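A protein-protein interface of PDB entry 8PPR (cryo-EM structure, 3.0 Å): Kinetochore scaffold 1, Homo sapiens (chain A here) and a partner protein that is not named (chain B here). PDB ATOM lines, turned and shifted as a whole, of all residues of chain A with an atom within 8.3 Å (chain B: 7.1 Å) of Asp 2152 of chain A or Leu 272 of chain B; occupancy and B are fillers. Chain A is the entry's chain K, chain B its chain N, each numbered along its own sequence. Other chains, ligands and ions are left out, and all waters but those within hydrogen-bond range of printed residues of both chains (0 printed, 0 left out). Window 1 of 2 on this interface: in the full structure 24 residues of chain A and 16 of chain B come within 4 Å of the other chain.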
ATOM      1  N   GLU A2134     -24.906  -0.845  11.248  1.00  0.00           N
ATOM      2  CA  GLU A2134     -24.456   0.539  11.147  1.00  0.00           C
ATOM      3  C   GLU A2134     -23.755   0.998  12.418  1.00  0.00           C
ATOM      4  O   GLU A2134     -22.757   1.725  12.354  1.00  0.00           O
ATOM      5  CB  GLU A2134     -25.645   1.451  10.837  1.00  0.00           C
ATOM      6  CG  GLU A2134     -25.301   2.932  10.792  1.00  0.00           C
ATOM      7  CD  GLU A2134     -24.389   3.286   9.637  1.00  0.00           C
ATOM      8  OE1 GLU A2134     -24.539   2.684   8.554  1.00  0.00           O
ATOM      9  OE2 GLU A2134     -23.521   4.167   9.814  1.00  0.00           O
ATOM     10  N   TRP A2135     -24.255   0.582  13.574  1.00  0.00           N
ATOM     11  CA  TRP A2135     -23.734   1.014  14.860  1.00  0.00           C
ATOM     12  C   TRP A2135     -22.749  -0.005  15.417  1.00  0.00           C
ATOM     13  O   TRP A2135     -22.786  -1.189  15.076  1.00  0.00           O
ATOM     14  CB  TRP A2135     -24.873   1.242  15.853  1.00  0.00           C
ATOM     15  CG  TRP A2135     -25.993   0.256  15.709  1.00  0.00           C
ATOM     16  CD1 TRP A2135     -27.183   0.462  15.077  1.00  0.00           C
ATOM     17  CD2 TRP A2135     -26.026  -1.092  16.195  1.00  0.00           C
ATOM     18  NE1 TRP A2135     -27.958  -0.669  15.142  1.00  0.00           N
ATOM     19  CE2 TRP A2135     -27.270  -1.639  15.824  1.00  0.00           C
ATOM     20  CE3 TRP A2135     -25.127  -1.888  16.910  1.00  0.00           C
ATOM     21  CZ2 TRP A2135     -27.636  -2.944  16.142  1.00  0.00           C
ATOM     22  CZ3 TRP A2135     -25.492  -3.184  17.223  1.00  0.00           C
ATOM     23  CH2 TRP A2135     -26.736  -3.699  16.841  1.00  0.00           C
ATOM     24  N   ASP A2136     -21.852   0.481  16.270  1.00  0.00           N
ATOM     25  CA  ASP A2136     -20.864  -0.345  16.948  1.00  0.00           C
ATOM     26  C   ASP A2136     -21.054  -0.193  18.448  1.00  0.00           C
ATOM     27  O   ASP A2136     -21.163   0.930  18.949  1.00  0.00           O
ATOM     28  CB  ASP A2136     -19.443   0.057  16.549  1.00  0.00           C
ATOM     29  CG  ASP A2136     -19.230   0.030  15.051  1.00  0.00           C
ATOM     30  OD1 ASP A2136     -19.833   0.871  14.351  1.00  0.00           O
ATOM     31  OD2 ASP A2136     -18.463  -0.831  14.574  1.00  0.00           O
ATOM     32  N   VAL A2137     -21.097  -1.314  19.156  1.00  0.00           N
ATOM     33  CA  VAL A2137     -21.329  -1.315  20.597  1.00  0.00           C
ATOM     34  C   VAL A2137     -19.971  -1.556  21.246  1.00  0.00           C
ATOM     35  O   VAL A2137     -19.541  -2.695  21.434  1.00  0.00           O
ATOM     36  CB  VAL A2137     -22.355  -2.362  21.012  1.00  0.00           C
ATOM     37  CG1 VAL A2137     -22.805  -2.107  22.441  1.00  0.00           C
ATOM     38  CG2 VAL A2137     -23.518  -2.389  20.040  1.00  0.00           C
ATOM     39  N   VAL A2138     -19.282  -0.470  21.589  1.00  0.00           N
ATOM     40  CA  VAL A2138     -17.973  -0.599  22.221  1.00  0.00           C
ATOM     41  C   VAL A2138     -18.114  -1.140  23.640  1.00  0.00           C
ATOM     42  O   VAL A2138     -17.373  -2.038  24.055  1.00  0.00           O
ATOM     43  CB  VAL A2138     -17.232   0.749  22.199  1.00  0.00           C
ATOM     44  CG1 VAL A2138     -16.061   0.727  23.164  1.00  0.00           C
ATOM     45  CG2 VAL A2138     -16.751   1.051  20.796  1.00  0.00           C
ATOM     46  N   PHE A2147     -22.559   3.333  22.423  1.00  0.00           N
ATOM     47  CA  PHE A2147     -22.550   3.071  20.993  1.00  0.00           C
ATOM     48  C   PHE A2147     -21.709   4.122  20.285  1.00  0.00           C
ATOM     49  O   PHE A2147     -21.735   5.304  20.635  1.00  0.00           O
ATOM     50  CB  PHE A2147     -23.967   3.077  20.416  1.00  0.00           C
ATOM     51  CG  PHE A2147     -24.858   2.017  20.985  1.00  0.00           C
ATOM     52  CD1 PHE A2147     -25.486   2.201  22.205  1.00  0.00           C
ATOM     53  CD2 PHE A2147     -25.086   0.843  20.290  1.00  0.00           C
ATOM     54  CE1 PHE A2147     -26.311   1.227  22.728  1.00  0.00           C
ATOM     55  CE2 PHE A2147     -25.915  -0.132  20.807  1.00  0.00           C
ATOM     56  CZ  PHE A2147     -26.525   0.058  22.027  1.00  0.00           C
ATOM     57  N   THR A2148     -20.965   3.679  19.274  1.00  0.00           N
ATOM     58  CA  THR A2148     -20.150   4.573  18.464  1.00  0.00           C
ATOM     59  C   THR A2148     -20.636   4.502  17.028  1.00  0.00           C
ATOM     60  O   THR A2148     -20.608   3.433  16.410  1.00  0.00           O
ATOM     61  CB  THR A2148     -18.666   4.212  18.546  1.00  0.00           C
ATOM     62  OG1 THR A2148     -18.450   2.927  17.947  1.00  0.00           O
ATOM     63  CG2 THR A2148     -18.208   4.188  19.993  1.00  0.00           C
ATOM     64  N   PHE A2149     -21.075   5.634  16.506  1.00  0.00           N
ATOM     65  CA  PHE A2149     -21.518   5.744  15.131  1.00  0.00           C
ATOM     66  C   PHE A2149     -20.341   6.156  14.255  1.00  0.00           C
ATOM     67  O   PHE A2149     -19.185   6.120  14.685  1.00  0.00           O
ATOM     68  CB  PHE A2149     -22.720   6.680  15.046  1.00  0.00           C
ATOM     69  CG  PHE A2149     -23.974   6.069  15.594  1.00  0.00           C
ATOM     70  CD1 PHE A2149     -24.268   6.144  16.945  1.00  0.00           C
ATOM     71  CD2 PHE A2149     -24.840   5.381  14.761  1.00  0.00           C
ATOM     72  CE1 PHE A2149     -25.417   5.565  17.449  1.00  0.00           C
ATOM     73  CE2 PHE A2149     -25.990   4.801  15.258  1.00  0.00           C
ATOM     74  CZ  PHE A2149     -26.279   4.891  16.604  1.00  0.00           C
ATOM     75  N   VAL A2150     -20.644   6.579  13.026  1.00  0.00           N
ATOM     76  CA  VAL A2150     -19.768   6.412  11.869  1.00  0.00           C
ATOM     77  C   VAL A2150     -18.305   6.673  12.196  1.00  0.00           C
ATOM     78  O   VAL A2150     -17.939   7.743  12.695  1.00  0.00           O
ATOM     79  CB  VAL A2150     -20.231   7.317  10.711  1.00  0.00           C
ATOM     80  CG1 VAL A2150     -21.572   6.850  10.197  1.00  0.00           C
ATOM     81  CG2 VAL A2150     -20.328   8.768  11.164  1.00  0.00           C
ATOM     82  N   TYR A2151     -17.471   5.671  11.915  1.00  0.00           N
ATOM     83  CA  TYR A2151     -16.023   5.745  12.095  1.00  0.00           C
ATOM     84  C   TYR A2151     -15.654   6.351  13.447  1.00  0.00           C
ATOM     85  O   TYR A2151     -14.727   7.156  13.566  1.00  0.00           O
ATOM     86  CB  TYR A2151     -15.393   6.500  10.928  1.00  0.00           C
ATOM     87  CG  TYR A2151     -15.975   6.041   9.609  1.00  0.00           C
ATOM     88  CD1 TYR A2151     -15.974   4.696   9.263  1.00  0.00           C
ATOM     89  CD2 TYR A2151     -16.568   6.935   8.736  1.00  0.00           C
ATOM     90  CE1 TYR A2151     -16.517   4.265   8.070  1.00  0.00           C
ATOM     91  CE2 TYR A2151     -17.118   6.515   7.543  1.00  0.00           C
ATOM     92  CZ  TYR A2151     -17.089   5.179   7.213  1.00  0.00           C
ATOM     93  OH  TYR A2151     -17.634   4.757   6.023  1.00  0.00           O
ATOM     94  N   ASP A2152     -16.409   5.959  14.475  1.00  0.00           N
ATOM     95  CA  ASP A2152     -16.119   6.257  15.876  1.00  0.00           C
ATOM     96  C   ASP A2152     -16.094   7.752  16.172  1.00  0.00           C
ATOM     97  O   ASP A2152     -15.473   8.181  17.151  1.00  0.00           O
ATOM     98  CB  ASP A2152     -14.801   5.610  16.311  1.00  0.00           C
ATOM     99  CG  ASP A2152     -14.860   4.098  16.281  1.00  0.00           C
ATOM    100  OD1 ASP A2152     -15.964   3.544  16.475  1.00  0.00           O
ATOM    101  OD2 ASP A2152     -13.809   3.463  16.058  1.00  0.00           O
ATOM    102  N   THR A2153     -16.757   8.562  15.353  1.00  0.00           N
ATOM    103  CA  THR A2153     -16.792  10.000  15.572  1.00  0.00           C
ATOM    104  C   THR A2153     -18.016  10.460  16.347  1.00  0.00           C
ATOM    105  O   THR A2153     -18.070  11.626  16.753  1.00  0.00           O
ATOM    106  CB  THR A2153     -16.740  10.739  14.234  1.00  0.00           C
ATOM    107  OG1 THR A2153     -17.867  10.358  13.435  1.00  0.00           O
ATOM    108  CG2 THR A2153     -15.468  10.385  13.507  1.00  0.00           C
ATOM    109  N   ILE A2154     -18.990   9.585  16.565  1.00  0.00           N
ATOM    110  CA  ILE A2154     -20.203   9.924  17.294  1.00  0.00           C
ATOM    111  C   ILE A2154     -20.399   8.897  18.394  1.00  0.00           C
ATOM    112  O   ILE A2154     -20.356   7.689  18.135  1.00  0.00           O
ATOM    113  CB  ILE A2154     -21.431   9.971  16.369  1.00  0.00           C
ATOM    114  CG1 ILE A2154     -21.281  11.113  15.364  1.00  0.00           C
ATOM    115  CG2 ILE A2154     -22.704  10.130  17.184  1.00  0.00           C
ATOM    116  CD1 ILE A2154     -22.487  11.313  14.487  1.00  0.00           C
ATOM    117  N   GLN A2155     -20.620   9.373  19.616  1.00  0.00           N
ATOM    118  CA  GLN A2155     -20.775   8.511  20.778  1.00  0.00           C
ATOM    119  C   GLN A2155     -22.217   8.566  21.251  1.00  0.00           C
ATOM    120  O   GLN A2155     -22.752   9.651  21.503  1.00  0.00           O
ATOM    121  CB  GLN A2155     -19.836   8.928  21.908  1.00  0.00           C
ATOM    122  CG  GLN A2155     -19.745   7.900  23.018  1.00  0.00           C
ATOM    123  CD  GLN A2155     -19.194   8.478  24.301  1.00  0.00           C
ATOM    124  OE1 GLN A2155     -19.815   9.338  24.923  1.00  0.00           O
ATOM    125  NE2 GLN A2155     -18.019   8.009  24.704  1.00  0.00           N
ATOM    126  N   GLN A2183     -22.882  12.409  21.764  1.00  0.00           N
ATOM    127  CA  GLN A2183     -21.643  13.169  21.760  1.00  0.00           C
ATOM    128  C   GLN A2183     -20.928  12.990  20.430  1.00  0.00           C
ATOM    129  O   GLN A2183     -21.086  11.980  19.741  1.00  0.00           O
ATOM    130  CB  GLN A2183     -20.726  12.759  22.919  1.00  0.00           C
ATOM    131  CG  GLN A2183     -21.000  13.524  24.202  1.00  0.00           C
ATOM    132  CD  GLN A2183     -20.048  13.156  25.317  1.00  0.00           C
ATOM    133  OE1 GLN A2183     -19.410  12.104  25.283  1.00  0.00           O
ATOM    134  NE2 GLN A2183     -19.945  14.023  26.318  1.00  0.00           N
ATOM    135  N   SER A2184     -20.131  13.996  20.083  1.00  0.00           N
ATOM    136  CA  SER A2184     -19.360  14.020  18.850  1.00  0.00           C
ATOM    137  C   SER A2184     -17.878  13.944  19.181  1.00  0.00           C
ATOM    138  O   SER A2184     -17.383  14.715  20.010  1.00  0.00           O
ATOM    139  CB  SER A2184     -19.655  15.285  18.045  1.00  0.00           C
ATOM    140  OG  SER A2184     -19.031  15.233  16.775  1.00  0.00           O
ATOM    141  N   LEU A2185     -17.177  13.017  18.535  1.00  0.00           N
ATOM    142  CA  LEU A2185     -15.748  12.836  18.740  1.00  0.00           C
ATOM    143  C   LEU A2185     -14.918  13.422  17.609  1.00  0.00           C
ATOM    144  O   LEU A2185     -13.699  13.226  17.580  1.00  0.00           O
ATOM    145  CB  LEU A2185     -15.434  11.350  18.907  1.00  0.00           C
ATOM    146  CG  LEU A2185     -16.038  10.718  20.163  1.00  0.00           C
ATOM    147  CD1 LEU A2185     -15.527   9.301  20.351  1.00  0.00           C
ATOM    148  CD2 LEU A2185     -15.745  11.572  21.387  1.00  0.00           C
ATOM    149  N   LEU A2186     -15.547  14.141  16.685  1.00  0.00           N
ATOM    150  CA  LEU A2186     -14.844  14.689  15.535  1.00  0.00           C
ATOM    151  C   LEU A2186     -13.954  15.854  15.950  1.00  0.00           C
ATOM    152  O   LEU A2186     -14.353  16.706  16.749  1.00  0.00           O
ATOM    153  CB  LEU A2186     -15.847  15.148  14.477  1.00  0.00           C
ATOM    154  CG  LEU A2186     -15.286  15.880  13.258  1.00  0.00           C
ATOM    155  CD1 LEU A2186     -14.489  14.926  12.386  1.00  0.00           C
ATOM    156  CD2 LEU A2186     -16.407  16.532  12.465  1.00  0.00           C
ATOM    157  N   ASP A2187     -12.745  15.887  15.396  1.00  0.00           N
ATOM    158  CA  ASP A2187     -11.804  16.978  15.639  1.00  0.00           C
ATOM    159  C   ASP A2187     -12.142  18.111  14.679  1.00  0.00           C
ATOM    160  O   ASP A2187     -11.710  18.113  13.525  1.00  0.00           O
ATOM    161  CB  ASP A2187     -10.367  16.504  15.463  1.00  0.00           C
ATOM    162  CG  ASP A2187      -9.369  17.409  16.151  1.00  0.00           C
ATOM    163  OD1 ASP A2187      -9.763  18.107  17.109  1.00  0.00           O
ATOM    164  OD2 ASP A2187      -8.193  17.427  15.734  1.00  0.00           O
ATOM    165  N   GLU A2188     -12.914  19.085  15.168  1.00  0.00           N
ATOM    166  CA  GLU A2188     -13.421  20.147  14.304  1.00  0.00           C
ATOM    167  C   GLU A2188     -12.302  21.013  13.743  1.00  0.00           C
ATOM    168  O   GLU A2188     -12.462  21.615  12.676  1.00  0.00           O
ATOM    169  CB  GLU A2188     -14.415  21.014  15.073  1.00  0.00           C
ATOM    170  CG  GLU A2188     -15.410  20.227  15.905  1.00  0.00           C
ATOM    171  CD  GLU A2188     -16.452  21.115  16.551  1.00  0.00           C
ATOM    172  OE1 GLU A2188     -17.343  21.612  15.831  1.00  0.00           O
ATOM    173  OE2 GLU A2188     -16.378  21.321  17.781  1.00  0.00           O
ATOM    174  N   GLN A2190      -9.403  20.218  12.442  1.00  0.00           N
ATOM    175  CA  GLN A2190      -8.888  19.665  11.198  1.00  0.00           C
ATOM    176  C   GLN A2190      -9.943  18.886  10.423  1.00  0.00           C
ATOM    177  O   GLN A2190      -9.600  18.174   9.473  1.00  0.00           O
ATOM    178  CB  GLN A2190      -7.677  18.781  11.494  1.00  0.00           C
ATOM    179  CG  GLN A2190      -7.995  17.601  12.391  1.00  0.00           C
ATOM    180  CD  GLN A2190      -6.768  16.791  12.743  1.00  0.00           C
ATOM    181  OE1 GLN A2190      -5.669  17.069  12.262  1.00  0.00           O
ATOM    182  NE2 GLN A2190      -6.943  15.792  13.598  1.00  0.00           N
ATOM    183  N   ALA A2191     -11.211  19.004  10.801  1.00  0.00           N
ATOM    184  CA  ALA A2191     -12.273  18.310  10.088  1.00  0.00           C
ATOM    185  C   ALA A2191     -12.579  19.018   8.769  1.00  0.00           C
ATOM    186  O   ALA A2191     -12.706  20.245   8.737  1.00  0.00           O
ATOM    187  CB  ALA A2191     -13.537  18.238  10.937  1.00  0.00           C
ATOM    188  N   HIS A2199     -21.942  16.042  10.682  1.00  0.00           N
ATOM    189  CA  HIS A2199     -22.175  16.068  12.122  1.00  0.00           C
ATOM    190  C   HIS A2199     -23.236  17.098  12.487  1.00  0.00           C
ATOM    191  O   HIS A2199     -24.094  16.842  13.340  1.00  0.00           O
ATOM    192  CB  HIS A2199     -20.869  16.342  12.859  1.00  0.00           C
ATOM    193  CG  HIS A2199     -20.062  15.111  13.119  1.00  0.00           C
ATOM    194  ND1 HIS A2199     -19.168  14.599  12.202  1.00  0.00           N
ATOM    195  CD2 HIS A2199     -20.034  14.271  14.181  1.00  0.00           C
ATOM    196  CE1 HIS A2199     -18.611  13.507  12.697  1.00  0.00           C
ATOM    197  NE2 HIS A2199     -19.119  13.287  13.896  1.00  0.00           N
ATOM    198  N   THR B 261     -11.593  -4.151  13.998  1.00  0.00           N
ATOM    199  CA  THR B 261     -11.390  -2.741  14.305  1.00  0.00           C
ATOM    200  C   THR B 261     -10.045  -2.314  13.731  1.00  0.00           C
ATOM    201  O   THR B 261      -9.007  -2.879  14.093  1.00  0.00           O
ATOM    202  CB  THR B 261     -11.441  -2.488  15.811  1.00  0.00           C
ATOM    203  OG1 THR B 261     -10.430  -3.267  16.462  1.00  0.00           O
ATOM    204  CG2 THR B 261     -12.805  -2.869  16.369  1.00  0.00           C
ATOM    205  N   LYS B 262     -10.066  -1.324  12.844  1.00  0.00           N
ATOM    206  CA  LYS B 262      -8.855  -0.897  12.156  1.00  0.00           C
ATOM    207  C   LYS B 262      -9.032   0.534  11.673  1.00  0.00           C
ATOM    208  O   LYS B 262     -10.140   1.076  11.665  1.00  0.00           O
ATOM    209  CB  LYS B 262      -8.526  -1.819  10.978  1.00  0.00           C
ATOM    210  CG  LYS B 262      -9.508  -1.709   9.824  1.00  0.00           C
ATOM    211  CD  LYS B 262      -9.244  -2.765   8.767  1.00  0.00           C
ATOM    212  CE  LYS B 262     -10.143  -2.564   7.559  1.00  0.00           C
ATOM    213  NZ  LYS B 262     -11.582  -2.707   7.913  1.00  0.00           N
ATOM    214  N   ASP B 263      -7.916   1.135  11.265  1.00  0.00           N
ATOM    215  CA  ASP B 263      -7.905   2.499  10.739  1.00  0.00           C
ATOM    216  C   ASP B 263      -8.434   2.466   9.311  1.00  0.00           C
ATOM    217  O   ASP B 263      -7.695   2.236   8.352  1.00  0.00           O
ATOM    218  CB  ASP B 263      -6.502   3.089  10.802  1.00  0.00           C
ATOM    219  CG  ASP B 263      -6.467   4.548  10.398  1.00  0.00           C
ATOM    220  OD1 ASP B 263      -6.911   5.397  11.199  1.00  0.00           O
ATOM    221  OD2 ASP B 263      -6.000   4.847   9.280  1.00  0.00           O
ATOM    222  N   CYS B 264      -9.735   2.701   9.170  1.00  0.00           N
ATOM    223  CA  CYS B 264     -10.366   2.685   7.863  1.00  0.00           C
ATOM    224  C   CYS B 264      -9.907   3.884   7.035  1.00  0.00           C
ATOM    225  O   CYS B 264      -9.480   4.901   7.584  1.00  0.00           O
ATOM    226  CB  CYS B 264     -11.884   2.700   8.012  1.00  0.00           C
ATOM    227  SG  CYS B 264     -12.516   4.096   8.970  1.00  0.00           S
ATOM    228  N   ARG B 267     -11.203   7.289   7.877  1.00  0.00           N
ATOM    229  CA  ARG B 267     -10.609   8.030   8.981  1.00  0.00           C
ATOM    230  C   ARG B 267      -9.911   9.294   8.501  1.00  0.00           C
ATOM    231  O   ARG B 267      -9.727  10.228   9.288  1.00  0.00           O
ATOM    232  CB  ARG B 267      -9.620   7.132   9.727  1.00  0.00           C
ATOM    233  CG  ARG B 267      -9.061   7.718  11.006  1.00  0.00           C
ATOM    234  CD  ARG B 267     -10.177   8.156  11.925  1.00  0.00           C
ATOM    235  NE  ARG B 267     -11.194   7.123  12.086  1.00  0.00           N
ATOM    236  CZ  ARG B 267     -11.060   6.051  12.855  1.00  0.00           C
ATOM    237  NH1 ARG B 267      -9.962   5.838  13.561  1.00  0.00           N
ATOM    238  NH2 ARG B 267     -12.055   5.171  12.918  1.00  0.00           N
ATOM    239  N   TYR B 270     -12.514  11.906   8.838  1.00  0.00           N
ATOM    240  CA  TYR B 270     -13.105  11.964  10.175  1.00  0.00           C
ATOM    241  C   TYR B 270     -12.012  11.824  11.224  1.00  0.00           C
ATOM    242  O   TYR B 270     -11.856  10.765  11.842  1.00  0.00           O
ATOM    243  CB  TYR B 270     -14.169  10.882  10.364  1.00  0.00           C
ATOM    244  CG  TYR B 270     -15.429  11.063   9.551  1.00  0.00           C
ATOM    245  CD1 TYR B 270     -15.719  12.269   8.941  1.00  0.00           C
ATOM    246  CD2 TYR B 270     -16.346  10.035   9.428  1.00  0.00           C
ATOM    247  CE1 TYR B 270     -16.874  12.439   8.205  1.00  0.00           C
ATOM    248  CE2 TYR B 270     -17.506  10.194   8.695  1.00  0.00           C
ATOM    249  CZ  TYR B 270     -17.764  11.400   8.086  1.00  0.00           C
ATOM    250  OH  TYR B 270     -18.916  11.573   7.355  1.00  0.00           O
ATOM    251  N   PRO B 271     -11.241  12.885  11.461  1.00  0.00           N
ATOM    252  CA  PRO B 271     -10.220  12.832  12.516  1.00  0.00           C
ATOM    253  C   PRO B 271     -10.867  12.895  13.892  1.00  0.00           C
ATOM    254  O   PRO B 271     -11.625  13.819  14.196  1.00  0.00           O
ATOM    255  CB  PRO B 271      -9.362  14.071  12.242  1.00  0.00           C
ATOM    256  CG  PRO B 271     -10.289  15.019  11.559  1.00  0.00           C
ATOM    257  CD  PRO B 271     -11.282  14.196  10.789  1.00  0.00           C
ATOM    258  N   LEU B 272     -10.570  11.901  14.723  1.00  0.00           N
ATOM    259  CA  LEU B 272     -11.076  11.904  16.087  1.00  0.00           C
ATOM    260  C   LEU B 272     -10.345  12.933  16.937  1.00  0.00           C
ATOM    261  O   LEU B 272      -9.187  13.279  16.685  1.00  0.00           O
ATOM    262  CB  LEU B 272     -10.947  10.522  16.730  1.00  0.00           C
ATOM    263  CG  LEU B 272     -11.963   9.438  16.362  1.00  0.00           C
ATOM    264  CD1 LEU B 272     -11.769   8.921  14.952  1.00  0.00           C
ATOM    265  CD2 LEU B 272     -11.892   8.295  17.366  1.00  0.00           C
ATOM    266  N   ARG B 273     -11.047  13.431  17.943  1.00  0.00           N
ATOM    267  CA  ARG B 273     -10.442  14.341  18.898  1.00  0.00           C
ATOM    268  C   ARG B 273      -9.403  13.598  19.735  1.00  0.00           C
ATOM    269  O   ARG B 273      -9.609  12.432  20.088  1.00  0.00           O
ATOM    270  CB  ARG B 273     -11.519  14.933  19.800  1.00  0.00           C
ATOM    271  CG  ARG B 273     -12.332  16.018  19.130  1.00  0.00           C
ATOM    272  CD  ARG B 273     -13.513  16.423  19.984  1.00  0.00           C
ATOM    273  NE  ARG B 273     -14.274  17.505  19.373  1.00  0.00           N
ATOM    274  CZ  ARG B 273     -15.375  18.029  19.893  1.00  0.00           C
ATOM    275  NH1 ARG B 273     -15.877  17.590  21.034  1.00  0.00           N
ATOM    276  NH2 ARG B 273     -15.989  19.017  19.247  1.00  0.00           N
ATOM    277  N   PRO B 274      -8.280  14.236  20.063  1.00  0.00           N
ATOM    278  CA  PRO B 274      -7.254  13.611  20.914  1.00  0.00           C
ATOM    279  C   PRO B 274      -7.567  13.739  22.405  1.00  0.00           C
ATOM    280  O   PRO B 274      -6.723  14.167  23.197  1.00  0.00           O
ATOM    281  CB  PRO B 274      -5.984  14.362  20.527  1.00  0.00           C
ATOM    282  CG  PRO B 274      -6.426  15.616  19.808  1.00  0.00           C
ATOM    283  CD  PRO B 274      -7.915  15.607  19.675  1.00  0.00           C
ATOM    284  N   LYS B 275      -8.794  13.381  22.784  1.00  0.00           N
ATOM    285  CA  LYS B 275      -9.340  13.451  24.138  1.00  0.00           C
ATOM    286  C   LYS B 275      -9.476  14.880  24.648  1.00  0.00           C
ATOM    287  O   LYS B 275      -9.952  15.071  25.775  1.00  0.00           O
ATOM    288  CB  LYS B 275      -8.521  12.640  25.153  1.00  0.00           C
ATOM    289  CG  LYS B 275      -8.172  11.235  24.694  1.00  0.00           C
ATOM    290  CD  LYS B 275      -9.428  10.432  24.401  1.00  0.00           C
ATOM    291  CE  LYS B 275      -9.198   8.948  24.629  1.00  0.00           C
ATOM    292  NZ  LYS B 275      -7.949   8.473  23.975  1.00  0.00           N
ATOM    293  N   LYS B 276      -9.092  15.883  23.860  1.00  0.00           N
ATOM    294  CA  LYS B 276      -9.154  17.291  24.253  1.00  0.00           C
ATOM    295  C   LYS B 276      -8.466  17.510  25.600  1.00  0.00           C
ATOM    296  O   LYS B 276      -9.064  17.966  26.577  1.00  0.00           O
ATOM    297  CB  LYS B 276     -10.603  17.788  24.281  1.00  0.00           C
ATOM    298  CG  LYS B 276     -11.387  17.521  23.001  1.00  0.00           C
ATOM    299  CD  LYS B 276     -10.556  17.798  21.755  1.00  0.00           C
ATOM    300  CE  LYS B 276     -10.688  19.241  21.304  1.00  0.00           C
ATOM    301  NZ  LYS B 276     -10.135  19.439  19.936  1.00  0.00           N
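The guanidinium group of Arg 267 of chain B lies within hydrogen-bond range of the backbone carbonyl oxygen of Tyr 2151 of chain A. The side-chain carboxylate (OD2) of Asp 2152 of chain A lies within salt-bridge range of the guanidinium group (NH2) of Arg 267 of chain B (3.98 Å). The backbone carbonyl oxygen (O) of Pro 271 of chain B lies within hydrogen-bond range of the backbone NH (N) of Asp 2187 of chain A, at 2.6 Å. O of Ser 2184 of chain A is in hydrogen-bond range of NH1 of Arg 273 of chain B, 3.4 Å away. The backbone NH (N) of Arg 273 of chain B lies within hydrogen-bond range of the backbone carbonyl oxygen (O) of Leu 2185 of chain A (2.7 Å). The guanidinium group of Arg 273 of chain B sits at hydrogen-bond distance from the backbone carbonyl oxygen of Leu 2186 of chain A (2.7 Å). NH2 of Arg 273 of chain B lies within salt-bridge range of OE2 of Glu 2188 of chain A, at 2.8 Å. The side-chain amino group (NZ) of Lys 276 of chain B is in salt-bridge range of the side-chain carboxylate (OD1) of Asp 2187 of chain A.
Of the 12 printed residues of chain B, 7 touch a printed residue of chain A. Printed residues of chain B that touch a printed residue of chain A: Cys 264, Arg 267, Tyr 270, Pro 271, Leu 272, Arg 273 and Lys 276. Hydrophobic or aromatic side chains of chain B within 4 Å of the printed part of chain A: Tyr 270, Pro 271 and Leu 272. Among the printed residues, Asp or Glu carboxylates within 4 Å of a Lys or Arg side-chain nitrogen of the other chain: Asp 2152 of chain A with Arg 267 of chain B (3.98 Å), Asp 2187 of chain A with Lys 276 of chain B (3.1 Å) and Glu 2188 of chain A with Arg 273 of chain B (2.8 Å).
Among the printed residues, pairs that only touch across the chains: Tyr 2151 of chain A with Cys 264 of chain B (3.5 Å), Tyr 2151 of chain A with Tyr 270 of chain B (3.2 Å), Tyr 2151 of chain A with Leu 272 of chain B (3.7 Å), Asp 2152 of chain A with Leu 272 of chain B (3.6 Å), Thr 2153 of chain A with Tyr 270 of chain B (3.4 Å), Leu 2185 of chain A with Leu 272 of chain B (3.3 Å), Leu 2186 of chain A with Tyr 270 of chain B (3.9 Å), Leu 2186 of chain A with Pro 271 of chain B (3.6 Å), Asp 2187 of chain A with Leu 272 of chain B (3.6 Å), Asp 2187 of chain A with Arg 273 of chain B (3.7 Å) and Gln 2190 of chain A with Pro 271 of chain B (3.3 Å).
Of the printed residues of chain B, Asp 2152 of chain A touches Arg 267 (3.98 Å) and Leu 272 (3.6 Å). Leu 272 of chain B touches just these residues of chain A: Tyr 2151 (3.7 Å), Asp 2152 (3.6 Å), Leu 2185 (3.3 Å) and Asp 2187 (3.6 Å). Printed residues of chain A within 4 Å of Arg 267 of chain B: Tyr 2151 and Asp 2152. Of the printed residues of chain B, Leu 2185 of chain A touches Leu 272 (3.3 Å) and Arg 273 (2.7 Å). Of the printed residues of chain B, Glu 2188 of chain A touches Arg 273. Printed residues of chain A within 4 Å of Lys 276 of chain B: Asp 2187. Of the printed residues of chain B, Thr 2153 of chain A touches Tyr 270 (3.4 Å). Glu 2134 of chain A touches none of the printed residues of chain B.
SG of Cys 264 of chain B sits at hydrogen-bond distance from N of Arg 267 of chain B (3.6 Å). The backbone carbonyl oxygen (O) of Val 2150 of chain A is in hydrogen-bond range of the side-chain hydroxyl (OG1) of Thr 2153 of chain A (2.7 Å). The backbone carbonyl oxygen of Thr 2153 of chain A lies within hydrogen-bond range of the backbone NH of Leu 2185 of chain A (2.4 Å). NE2 of His 2199 of chain A lies close to OG of Ser 2184 of chain A (3.5 Å).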
